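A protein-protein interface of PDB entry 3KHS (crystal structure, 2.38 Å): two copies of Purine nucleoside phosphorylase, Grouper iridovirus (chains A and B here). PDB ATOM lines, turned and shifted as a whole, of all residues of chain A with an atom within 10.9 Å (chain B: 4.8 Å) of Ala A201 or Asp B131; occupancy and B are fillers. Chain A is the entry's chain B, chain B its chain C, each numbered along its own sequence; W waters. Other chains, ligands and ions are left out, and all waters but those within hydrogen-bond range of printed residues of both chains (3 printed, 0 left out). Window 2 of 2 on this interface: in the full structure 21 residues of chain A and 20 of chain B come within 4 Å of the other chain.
The backbone carbonyl oxygen (O) of His B132 sits at hydrogen-bond distance from the side-chain hydroxyl (OG1) of Thr A199 (2.7 Å). N of Ala A201 is in hydrogen-bond range of OD2 of Asp B131 (2.9 Å).
The backbone carbonyl oxygen (O) of Asp B131 is in hydrogen-bond range of the backbone NH (N) of Tyr B189, 2.9 Å away. N of Ile B133 is in hydrogen-bond range of O of Tyr B189, at 2.9 Å. SG of Cys A246 is disulfide-bonded to SG of Cys A203 (2.0 Å). The side-chain hydroxyl (OH) of Tyr B163 is in hydrogen-bond range of a ring nitrogen (ND1) of His B132, at 2.8 Å. OE1 of Glu A202 sits at hydrogen-bond distance from N of Thr A199 (2.8 Å).
CB of Thr A199 touches OD1 of Asp B131, 3.2 Å away. Pro A200 touches Asp B131 (CD to OD2, 3.2 Å). O of His B132 touches CB of Ala A201 (3.8 Å). Ile B133 touches Ala A201 (CG1 to CB, 3.95 Å). OE2 of Glu A202 touches CD2 of His B132, 3.7 Å away. OE2 of Glu A202 touches C of Ile B133, 3.7 Å away. Ile B133 touches Ile A205. Met B209 touches Ile A205.
Of chain B, only Asp B131 (2.9 Å), His B132 (3.8 Å) and Ile B133 (3.95 Å) come within 4 Å of Ala A201. Of the printed residues of chain B, Ile A205 touches Ile B133 (3.5 Å) and Met B209 (3.7 Å). No residue of chain A comes within 4 Å of Val B129. No residue of chain A comes within 4 Å of Arg B130. Printed residues of chain A within 4 Å of Asp B131: Thr A199, Pro A200 and Ala A201. No residue of chain A comes within 4 Å of Gly B187. Of the printed residues of chain A, Met B209 touches Ile A205 (3.7 Å). The nearest residue of chain A that does not touch Asp B131 is Glu A202 (5.1 Å).
Of the 10 printed residues of chain B, 4 touch a printed residue of chain A. Hydrophobic or aromatic side chains of chain A within 4 Å of the printed part of chain B: Pro A200, Ala A201 and Ile A205. Among the printed residues, no Asp or Glu carboxylate lies within 4 Å of a Lys or Arg side-chain nitrogen of the other chain.
Position printed for both chains: 209. Of the 10 pairs that touch across the chains among the printed residues, none has its exchanged pair printed and touching as well.
Water W1 lies within hydrogen-bond range of O of Met B209 and O of Ala A201. Water W3 lies within hydrogen-bond range of OD2 of Asp B131 (2.7 Å), NH2 of Arg B130 (3.2 Å) and N of Ala A201 (3.5 Å). Water W2 lies within hydrogen-bond range of NE2 of His B132 and OE2 of Glu A202.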
ATOM      1  N   LEU A 117       9.750  26.120 -26.321  1.00  0.00           N
ATOM      2  CA  LEU A 117       9.862  24.679 -26.217  1.00  0.00           C
ATOM      3  C   LEU A 117      10.522  24.176 -27.509  1.00  0.00           C
ATOM      4  O   LEU A 117      11.233  23.172 -27.504  1.00  0.00           O
ATOM      5  CB  LEU A 117       8.469  24.075 -26.057  1.00  0.00           C
ATOM      6  CG  LEU A 117       7.765  24.461 -24.738  1.00  0.00           C
ATOM      7  CD1 LEU A 117       6.278  24.268 -24.844  1.00  0.00           C
ATOM      8  CD2 LEU A 117       8.336  23.627 -23.575  1.00  0.00           C
ATOM      9  N   LEU A 135      -5.457  25.088 -22.822  1.00  0.00           N
ATOM     10  CA  LEU A 135      -5.860  24.071 -21.845  1.00  0.00           C
ATOM     11  C   LEU A 135      -6.969  24.494 -20.875  1.00  0.00           C
ATOM     12  O   LEU A 135      -7.935  23.782 -20.710  1.00  0.00           O
ATOM     13  CB  LEU A 135      -4.634  23.578 -21.078  1.00  0.00           C
ATOM     14  CG  LEU A 135      -3.546  22.970 -21.997  1.00  0.00           C
ATOM     15  CD1 LEU A 135      -2.291  22.740 -21.176  1.00  0.00           C
ATOM     16  CD2 LEU A 135      -4.025  21.645 -22.653  1.00  0.00           C
ATOM     17  N   PHE A 197       5.373  27.425 -12.946  1.00  0.00           N
ATOM     18  CA  PHE A 197       5.870  26.911 -14.206  1.00  0.00           C
ATOM     19  C   PHE A 197       5.646  25.420 -14.159  1.00  0.00           C
ATOM     20  O   PHE A 197       5.440  24.843 -13.068  1.00  0.00           O
ATOM     21  CB  PHE A 197       7.352  27.255 -14.392  1.00  0.00           C
ATOM     22  CG  PHE A 197       7.593  28.723 -14.687  1.00  0.00           C
ATOM     23  CD1 PHE A 197       6.915  29.357 -15.740  1.00  0.00           C
ATOM     24  CD2 PHE A 197       8.507  29.469 -13.936  1.00  0.00           C
ATOM     25  CE1 PHE A 197       7.145  30.709 -16.043  1.00  0.00           C
ATOM     26  CE2 PHE A 197       8.745  30.827 -14.229  1.00  0.00           C
ATOM     27  CZ  PHE A 197       8.060  31.443 -15.284  1.00  0.00           C
ATOM     28  N   GLU A 198       5.654  24.780 -15.319  1.00  0.00           N
ATOM     29  CA  GLU A 198       5.381  23.355 -15.344  1.00  0.00           C
ATOM     30  C   GLU A 198       6.537  22.438 -14.933  1.00  0.00           C
ATOM     31  O   GLU A 198       7.724  22.814 -15.003  1.00  0.00           O
ATOM     32  CB  GLU A 198       4.851  22.921 -16.717  1.00  0.00           C
ATOM     33  CG  GLU A 198       5.390  23.629 -17.930  1.00  0.00           C
ATOM     34  CD  GLU A 198       4.820  25.044 -18.145  1.00  0.00           C
ATOM     35  OE1 GLU A 198       3.608  25.297 -17.888  1.00  0.00           O
ATOM     36  OE2 GLU A 198       5.611  25.912 -18.585  1.00  0.00           O
ATOM     37  N   THR A 199       6.182  21.238 -14.467  1.00  0.00           N
ATOM     38  CA  THR A 199       7.208  20.287 -14.097  1.00  0.00           C
ATOM     39  C   THR A 199       7.785  19.720 -15.380  1.00  0.00           C
ATOM     40  O   THR A 199       7.211  19.895 -16.461  1.00  0.00           O
ATOM     41  CB  THR A 199       6.667  19.134 -13.279  1.00  0.00           C
ATOM     42  OG1 THR A 199       5.650  18.453 -14.018  1.00  0.00           O
ATOM     43  CG2 THR A 199       6.148  19.634 -11.946  1.00  0.00           C
ATOM     44  N   PRO A 200       8.953  19.054 -15.287  1.00  0.00           N
ATOM     45  CA  PRO A 200       9.543  18.485 -16.502  1.00  0.00           C
ATOM     46  C   PRO A 200       8.574  17.484 -17.136  1.00  0.00           C
ATOM     47  O   PRO A 200       8.430  17.426 -18.359  1.00  0.00           O
ATOM     48  CB  PRO A 200      10.820  17.815 -15.992  1.00  0.00           C
ATOM     49  CG  PRO A 200      11.215  18.696 -14.852  1.00  0.00           C
ATOM     50  CD  PRO A 200       9.875  18.919 -14.150  1.00  0.00           C
ATOM     51  N   ALA A 201       7.912  16.698 -16.306  1.00  0.00           N
ATOM     52  CA  ALA A 201       6.957  15.742 -16.834  1.00  0.00           C
ATOM     53  C   ALA A 201       5.779  16.436 -17.544  1.00  0.00           C
ATOM     54  O   ALA A 201       5.225  15.890 -18.499  1.00  0.00           O
ATOM     55  CB  ALA A 201       6.447  14.846 -15.733  1.00  0.00           C
ATOM     56  N   GLU A 202       5.391  17.620 -17.080  1.00  0.00           N
ATOM     57  CA  GLU A 202       4.287  18.354 -17.718  1.00  0.00           C
ATOM     58  C   GLU A 202       4.775  18.961 -19.037  1.00  0.00           C
ATOM     59  O   GLU A 202       4.080  18.957 -20.039  1.00  0.00           O
ATOM     60  CB  GLU A 202       3.761  19.447 -16.785  1.00  0.00           C
ATOM     61  CG  GLU A 202       2.971  18.874 -15.634  1.00  0.00           C
ATOM     62  CD  GLU A 202       2.804  19.819 -14.470  1.00  0.00           C
ATOM     63  OE1 GLU A 202       3.445  20.888 -14.464  1.00  0.00           O
ATOM     64  OE2 GLU A 202       2.036  19.475 -13.542  1.00  0.00           O
ATOM     65  N   CYS A 203       5.999  19.458 -19.018  1.00  0.00           N
ATOM     66  CA  CYS A 203       6.624  20.074 -20.181  1.00  0.00           C
ATOM     67  C   CYS A 203       6.672  19.034 -21.295  1.00  0.00           C
ATOM     68  O   CYS A 203       6.412  19.332 -22.455  1.00  0.00           O
ATOM     69  CB  CYS A 203       8.004  20.560 -19.786  1.00  0.00           C
ATOM     70  SG  CYS A 203       9.178  20.961 -21.095  1.00  0.00           S
ATOM     71  N   LYS A 204       6.971  17.800 -20.935  1.00  0.00           N
ATOM     72  CA  LYS A 204       7.000  16.733 -21.911  1.00  0.00           C
ATOM     73  C   LYS A 204       5.647  16.588 -22.548  1.00  0.00           C
ATOM     74  O   LYS A 204       5.549  16.441 -23.754  1.00  0.00           O
ATOM     75  CB  LYS A 204       7.386  15.413 -21.260  1.00  0.00           C
ATOM     76  CG  LYS A 204       8.875  15.346 -20.990  1.00  0.00           C
ATOM     77  CD  LYS A 204       9.268  14.134 -20.170  1.00  0.00           C
ATOM     78  CE  LYS A 204      10.714  14.277 -19.738  1.00  0.00           C
ATOM     79  NZ  LYS A 204      11.228  13.066 -19.044  1.00  0.00           N
ATOM     80  N   ILE A 205       4.594  16.619 -21.743  1.00  0.00           N
ATOM     81  CA  ILE A 205       3.260  16.488 -22.293  1.00  0.00           C
ATOM     82  C   ILE A 205       2.958  17.647 -23.260  1.00  0.00           C
ATOM     83  O   ILE A 205       2.385  17.449 -24.335  1.00  0.00           O
ATOM     84  CB  ILE A 205       2.246  16.453 -21.181  1.00  0.00           C
ATOM     85  CG1 ILE A 205       2.413  15.147 -20.393  1.00  0.00           C
ATOM     86  CG2 ILE A 205       0.863  16.615 -21.762  1.00  0.00           C
ATOM     87  CD1 ILE A 205       1.853  15.216 -18.920  1.00  0.00           C
ATOM     88  N   LEU A 206       3.395  18.844 -22.905  1.00  0.00           N
ATOM     89  CA  LEU A 206       3.162  20.001 -23.751  1.00  0.00           C
ATOM     90  C   LEU A 206       3.861  19.846 -25.104  1.00  0.00           C
ATOM     91  O   LEU A 206       3.357  20.329 -26.125  1.00  0.00           O
ATOM     92  CB  LEU A 206       3.645  21.259 -23.060  1.00  0.00           C
ATOM     93  CG  LEU A 206       2.599  22.039 -22.273  1.00  0.00           C
ATOM     94  CD1 LEU A 206       1.715  21.130 -21.436  1.00  0.00           C
ATOM     95  CD2 LEU A 206       3.316  23.077 -21.435  1.00  0.00           C
ATOM     96  N   ARG A 207       5.024  19.187 -25.109  1.00  0.00           N
ATOM     97  CA  ARG A 207       5.765  18.966 -26.341  1.00  0.00           C
ATOM     98  C   ARG A 207       5.037  17.924 -27.128  1.00  0.00           C
ATOM     99  O   ARG A 207       4.893  18.032 -28.339  1.00  0.00           O
ATOM    100  CB  ARG A 207       7.165  18.467 -26.068  1.00  0.00           C
ATOM    101  CG  ARG A 207       8.077  19.572 -25.714  1.00  0.00           C
ATOM    102  CD  ARG A 207       9.491  19.107 -25.594  1.00  0.00           C
ATOM    103  NE  ARG A 207      10.295  20.294 -25.442  1.00  0.00           N
ATOM    104  CZ  ARG A 207      11.550  20.290 -25.043  1.00  0.00           C
ATOM    105  NH1 ARG A 207      12.143  19.135 -24.760  1.00  0.00           N
ATOM    106  NH2 ARG A 207      12.193  21.445 -24.898  1.00  0.00           N
ATOM    107  N   LEU A 208       4.567  16.902 -26.439  1.00  0.00           N
ATOM    108  CA  LEU A 208       3.834  15.856 -27.111  1.00  0.00           C
ATOM    109  C   LEU A 208       2.569  16.466 -27.748  1.00  0.00           C
ATOM    110  O   LEU A 208       2.066  15.929 -28.722  1.00  0.00           O
ATOM    111  CB  LEU A 208       3.480  14.776 -26.099  1.00  0.00           C
ATOM    112  CG  LEU A 208       2.981  13.392 -26.500  1.00  0.00           C
ATOM    113  CD1 LEU A 208       3.537  12.941 -27.850  1.00  0.00           C
ATOM    114  CD2 LEU A 208       3.431  12.424 -25.389  1.00  0.00           C
ATOM    115  N   MET A 209       2.056  17.580 -27.216  1.00  0.00           N
ATOM    116  CA  MET A 209       0.850  18.181 -27.818  1.00  0.00           C
ATOM    117  C   MET A 209       1.170  19.070 -29.019  1.00  0.00           C
ATOM    118  O   MET A 209       0.267  19.574 -29.677  1.00  0.00           O
ATOM    119  CB  MET A 209       0.054  18.991 -26.786  1.00  0.00           C
ATOM    120  CG  MET A 209      -0.789  18.163 -25.869  1.00  0.00           C
ATOM    121  SD  MET A 209      -1.220  19.071 -24.364  1.00  0.00           S
ATOM    122  CE  MET A 209      -2.401  17.848 -23.625  1.00  0.00           C
ATOM    123  N   ILE A 242      13.464  26.233 -22.932  1.00  0.00           N
ATOM    124  CA  ILE A 242      13.540  25.031 -22.135  1.00  0.00           C
ATOM    125  C   ILE A 242      14.450  24.056 -22.846  1.00  0.00           C
ATOM    126  O   ILE A 242      14.324  23.874 -24.049  1.00  0.00           O
ATOM    127  CB  ILE A 242      12.139  24.420 -21.981  1.00  0.00           C
ATOM    128  CG1 ILE A 242      11.265  25.325 -21.104  1.00  0.00           C
ATOM    129  CG2 ILE A 242      12.231  23.023 -21.390  1.00  0.00           C
ATOM    130  CD1 ILE A 242      10.719  26.574 -21.777  1.00  0.00           C
ATOM    131  N   ALA A 243      15.375  23.440 -22.119  1.00  0.00           N
ATOM    132  CA  ALA A 243      16.283  22.482 -22.744  1.00  0.00           C
ATOM    133  C   ALA A 243      15.544  21.217 -23.174  1.00  0.00           C
ATOM    134  O   ALA A 243      14.380  21.018 -22.844  1.00  0.00           O
ATOM    135  CB  ALA A 243      17.413  22.124 -21.790  1.00  0.00           C
ATOM    136  N   SER A 244      16.236  20.363 -23.910  1.00  0.00           N
ATOM    137  CA  SER A 244      15.648  19.130 -24.397  1.00  0.00           C
ATOM    138  C   SER A 244      15.120  18.226 -23.293  1.00  0.00           C
ATOM    139  O   SER A 244      14.146  17.522 -23.511  1.00  0.00           O
ATOM    140  CB  SER A 244      16.661  18.374 -25.260  1.00  0.00           C
ATOM    141  OG  SER A 244      17.903  18.246 -24.594  1.00  0.00           O
ATOM    142  N   ASN A 245      15.745  18.245 -22.117  1.00  0.00           N
ATOM    143  CA  ASN A 245      15.299  17.406 -21.001  1.00  0.00           C
ATOM    144  C   ASN A 245      14.045  17.975 -20.320  1.00  0.00           C
ATOM    145  O   ASN A 245      13.534  17.404 -19.344  1.00  0.00           O
ATOM    146  CB  ASN A 245      16.415  17.270 -19.975  1.00  0.00           C
ATOM    147  CG  ASN A 245      16.836  18.601 -19.429  1.00  0.00           C
ATOM    148  OD1 ASN A 245      16.549  19.635 -20.032  1.00  0.00           O
ATOM    149  ND2 ASN A 245      17.528  18.597 -18.293  1.00  0.00           N
ATOM    150  N   CYS A 246      13.569  19.102 -20.851  1.00  0.00           N
ATOM    151  CA  CYS A 246      12.385  19.793 -20.366  1.00  0.00           C
ATOM    152  C   CYS A 246      12.510  20.471 -18.985  1.00  0.00           C
ATOM    153  O   CYS A 246      11.654  20.304 -18.121  1.00  0.00           O
ATOM    154  CB  CYS A 246      11.192  18.836 -20.382  1.00  0.00           C
ATOM    155  SG  CYS A 246       9.932  19.149 -21.667  1.00  0.00           S
ATOM    156  N   GLU A 247      13.564  21.258 -18.794  1.00  0.00           N
ATOM    157  CA  GLU A 247      13.765  21.975 -17.538  1.00  0.00           C
ATOM    158  C   GLU A 247      14.100  23.437 -17.813  1.00  0.00           C
ATOM    159  O   GLU A 247      14.645  23.763 -18.870  1.00  0.00           O
ATOM    160  CB  GLU A 247      14.893  21.330 -16.743  1.00  0.00           C
ATOM    161  CG  GLU A 247      14.780  19.828 -16.641  1.00  0.00           C
ATOM    162  CD  GLU A 247      15.796  19.253 -15.681  1.00  0.00           C
ATOM    163  OE1 GLU A 247      16.937  19.778 -15.655  1.00  0.00           O
ATOM    164  OE2 GLU A 247      15.459  18.278 -14.968  1.00  0.00           O
ATOM    165  N   VAL B 129       7.944   9.471  -5.181  1.00  0.00           N
ATOM    166  CA  VAL B 129       7.668  10.392  -6.270  1.00  0.00           C
ATOM    167  C   VAL B 129       8.851  11.222  -6.759  1.00  0.00           C
ATOM    168  O   VAL B 129       9.450  11.989  -5.999  1.00  0.00           O
ATOM    169  CB  VAL B 129       6.530  11.363  -5.898  1.00  0.00           C
ATOM    170  CG1 VAL B 129       6.092  12.176  -7.150  1.00  0.00           C
ATOM    171  CG2 VAL B 129       5.374  10.584  -5.323  1.00  0.00           C
ATOM    172  N   ARG B 130       9.183  11.081  -8.042  1.00  0.00           N
ATOM    173  CA  ARG B 130      10.287  11.854  -8.595  1.00  0.00           C
ATOM    174  C   ARG B 130       9.788  13.072  -9.383  1.00  0.00           C
ATOM    175  O   ARG B 130      10.549  14.008  -9.625  1.00  0.00           O
ATOM    176  CB  ARG B 130      11.195  10.995  -9.479  1.00  0.00           C
ATOM    177  CG  ARG B 130      10.489   9.867 -10.221  1.00  0.00           C
ATOM    178  CD  ARG B 130      11.335   9.339 -11.396  1.00  0.00           C
ATOM    179  NE  ARG B 130      11.381  10.359 -12.426  1.00  0.00           N
ATOM    180  CZ  ARG B 130      10.942  10.200 -13.663  1.00  0.00           C
ATOM    181  NH1 ARG B 130      10.439   9.041 -14.046  1.00  0.00           N
ATOM    182  NH2 ARG B 130      10.936  11.234 -14.485  1.00  0.00           N
ATOM    183  N   ASP B 131       8.523  13.053  -9.790  1.00  0.00           N
ATOM    184  CA  ASP B 131       7.940  14.191 -10.501  1.00  0.00           C
ATOM    185  C   ASP B 131       6.421  13.990 -10.584  1.00  0.00           C
ATOM    186  O   ASP B 131       5.917  12.904 -10.267  1.00  0.00           O
ATOM    187  CB  ASP B 131       8.538  14.316 -11.911  1.00  0.00           C
ATOM    188  CG  ASP B 131       8.349  15.706 -12.514  1.00  0.00           C
ATOM    189  OD1 ASP B 131       7.827  16.588 -11.809  1.00  0.00           O
ATOM    190  OD2 ASP B 131       8.741  15.930 -13.677  1.00  0.00           O
ATOM    191  N   HIS B 132       5.684  15.025 -10.998  1.00  0.00           N
ATOM    192  CA  HIS B 132       4.242  14.886 -11.111  1.00  0.00           C
ATOM    193  C   HIS B 132       3.663  15.564 -12.322  1.00  0.00           C
ATOM    194  O   HIS B 132       4.324  16.344 -13.008  1.00  0.00           O
ATOM    195  CB  HIS B 132       3.506  15.367  -9.831  1.00  0.00           C
ATOM    196  CG  HIS B 132       3.509  16.853  -9.616  1.00  0.00           C
ATOM    197  ND1 HIS B 132       3.817  17.422  -8.397  1.00  0.00           N
ATOM    198  CD2 HIS B 132       3.227  17.886 -10.447  1.00  0.00           C
ATOM    199  CE1 HIS B 132       3.734  18.738  -8.490  1.00  0.00           C
ATOM    200  NE2 HIS B 132       3.380  19.046  -9.723  1.00  0.00           N
ATOM    201  N   ILE B 133       2.407  15.234 -12.580  1.00  0.00           N
ATOM    202  CA  ILE B 133       1.648  15.781 -13.684  1.00  0.00           C
ATOM    203  C   ILE B 133       0.376  16.215 -12.996  1.00  0.00           C
ATOM    204  O   ILE B 133      -0.422  15.372 -12.575  1.00  0.00           O
ATOM    205  CB  ILE B 133       1.296  14.701 -14.721  1.00  0.00           C
ATOM    206  CG1 ILE B 133       2.568  14.170 -15.397  1.00  0.00           C
ATOM    207  CG2 ILE B 133       0.286  15.265 -15.718  1.00  0.00           C
ATOM    208  CD1 ILE B 133       2.283  12.929 -16.269  1.00  0.00           C
ATOM    209  N   TYR B 163      10.384  17.555  -6.274  1.00  0.00           N
ATOM    210  CA  TYR B 163      10.794  16.478  -5.365  1.00  0.00           C
ATOM    211  C   TYR B 163      12.312  16.389  -5.124  1.00  0.00           C
ATOM    212  O   TYR B 163      13.065  15.892  -5.965  1.00  0.00           O
ATOM    213  CB  TYR B 163      10.231  15.155  -5.902  1.00  0.00           C
ATOM    214  CG  TYR B 163       8.706  15.233  -6.003  1.00  0.00           C
ATOM    215  CD1 TYR B 163       7.904  15.081  -4.871  1.00  0.00           C
ATOM    216  CD2 TYR B 163       8.083  15.618  -7.196  1.00  0.00           C
ATOM    217  CE1 TYR B 163       6.528  15.324  -4.923  1.00  0.00           C
ATOM    218  CE2 TYR B 163       6.718  15.859  -7.259  1.00  0.00           C
ATOM    219  CZ  TYR B 163       5.947  15.711  -6.112  1.00  0.00           C
ATOM    220  OH  TYR B 163       4.596  15.946  -6.164  1.00  0.00           O
ATOM    221  N   GLY B 187       8.883   6.923  -9.392  1.00  0.00           N
ATOM    222  CA  GLY B 187       8.179   7.262 -10.611  1.00  0.00           C
ATOM    223  C   GLY B 187       7.400   8.554 -10.618  1.00  0.00           C
ATOM    224  O   GLY B 187       7.497   9.373  -9.692  1.00  0.00           O
ATOM    225  N   VAL B 188       6.611   8.720 -11.676  1.00  0.00           N
ATOM    226  CA  VAL B 188       5.817   9.917 -11.896  1.00  0.00           C
ATOM    227  C   VAL B 188       4.392   9.818 -11.376  1.00  0.00           C
ATOM    228  O   VAL B 188       3.661   8.895 -11.743  1.00  0.00           O
ATOM    229  CB  VAL B 188       5.770  10.228 -13.402  1.00  0.00           C
ATOM    230  CG1 VAL B 188       4.885  11.463 -13.676  1.00  0.00           C
ATOM    231  CG2 VAL B 188       7.196  10.405 -13.928  1.00  0.00           C
ATOM    232  N   TYR B 189       3.996  10.770 -10.531  1.00  0.00           N
ATOM    233  CA  TYR B 189       2.626  10.767  -9.987  1.00  0.00           C
ATOM    234  C   TYR B 189       1.711  11.698 -10.786  1.00  0.00           C
ATOM    235  O   TYR B 189       2.017  12.863 -10.967  1.00  0.00           O
ATOM    236  CB  TYR B 189       2.632  11.208  -8.507  1.00  0.00           C
ATOM    237  CG  TYR B 189       1.280  11.290  -7.840  1.00  0.00           C
ATOM    238  CD1 TYR B 189       0.816  10.249  -7.038  1.00  0.00           C
ATOM    239  CD2 TYR B 189       0.467  12.413  -7.998  1.00  0.00           C
ATOM    240  CE1 TYR B 189      -0.437  10.318  -6.387  1.00  0.00           C
ATOM    241  CE2 TYR B 189      -0.780  12.493  -7.369  1.00  0.00           C
ATOM    242  CZ  TYR B 189      -1.221  11.445  -6.558  1.00  0.00           C
ATOM    243  OH  TYR B 189      -2.427  11.541  -5.881  1.00  0.00           O
ATOM    244  N   MET B 209       0.767   9.944 -21.256  1.00  0.00           N
ATOM    245  CA  MET B 209       1.447  11.108 -20.684  1.00  0.00           C
ATOM    246  C   MET B 209       2.679  10.715 -19.861  1.00  0.00           C
ATOM    247  O   MET B 209       3.429  11.581 -19.408  1.00  0.00           O
ATOM    248  CB  MET B 209       0.479  11.906 -19.797  1.00  0.00           C
ATOM    249  CG  MET B 209      -0.496  12.786 -20.554  1.00  0.00           C
ATOM    250  SD  MET B 209      -1.826  13.381 -19.484  1.00  0.00           S
ATOM    251  CE  MET B 209      -2.652  14.466 -20.641  1.00  0.00           C
HETATM  252  O   HOH W   1       5.252  13.290 -18.911  1.00  0.00           O
HETATM  253  O   HOH W   2       2.807  21.145 -11.426  1.00  0.00           O
HETATM  254  O   HOH W   3      10.044  14.175 -15.207  1.00  0.00           O
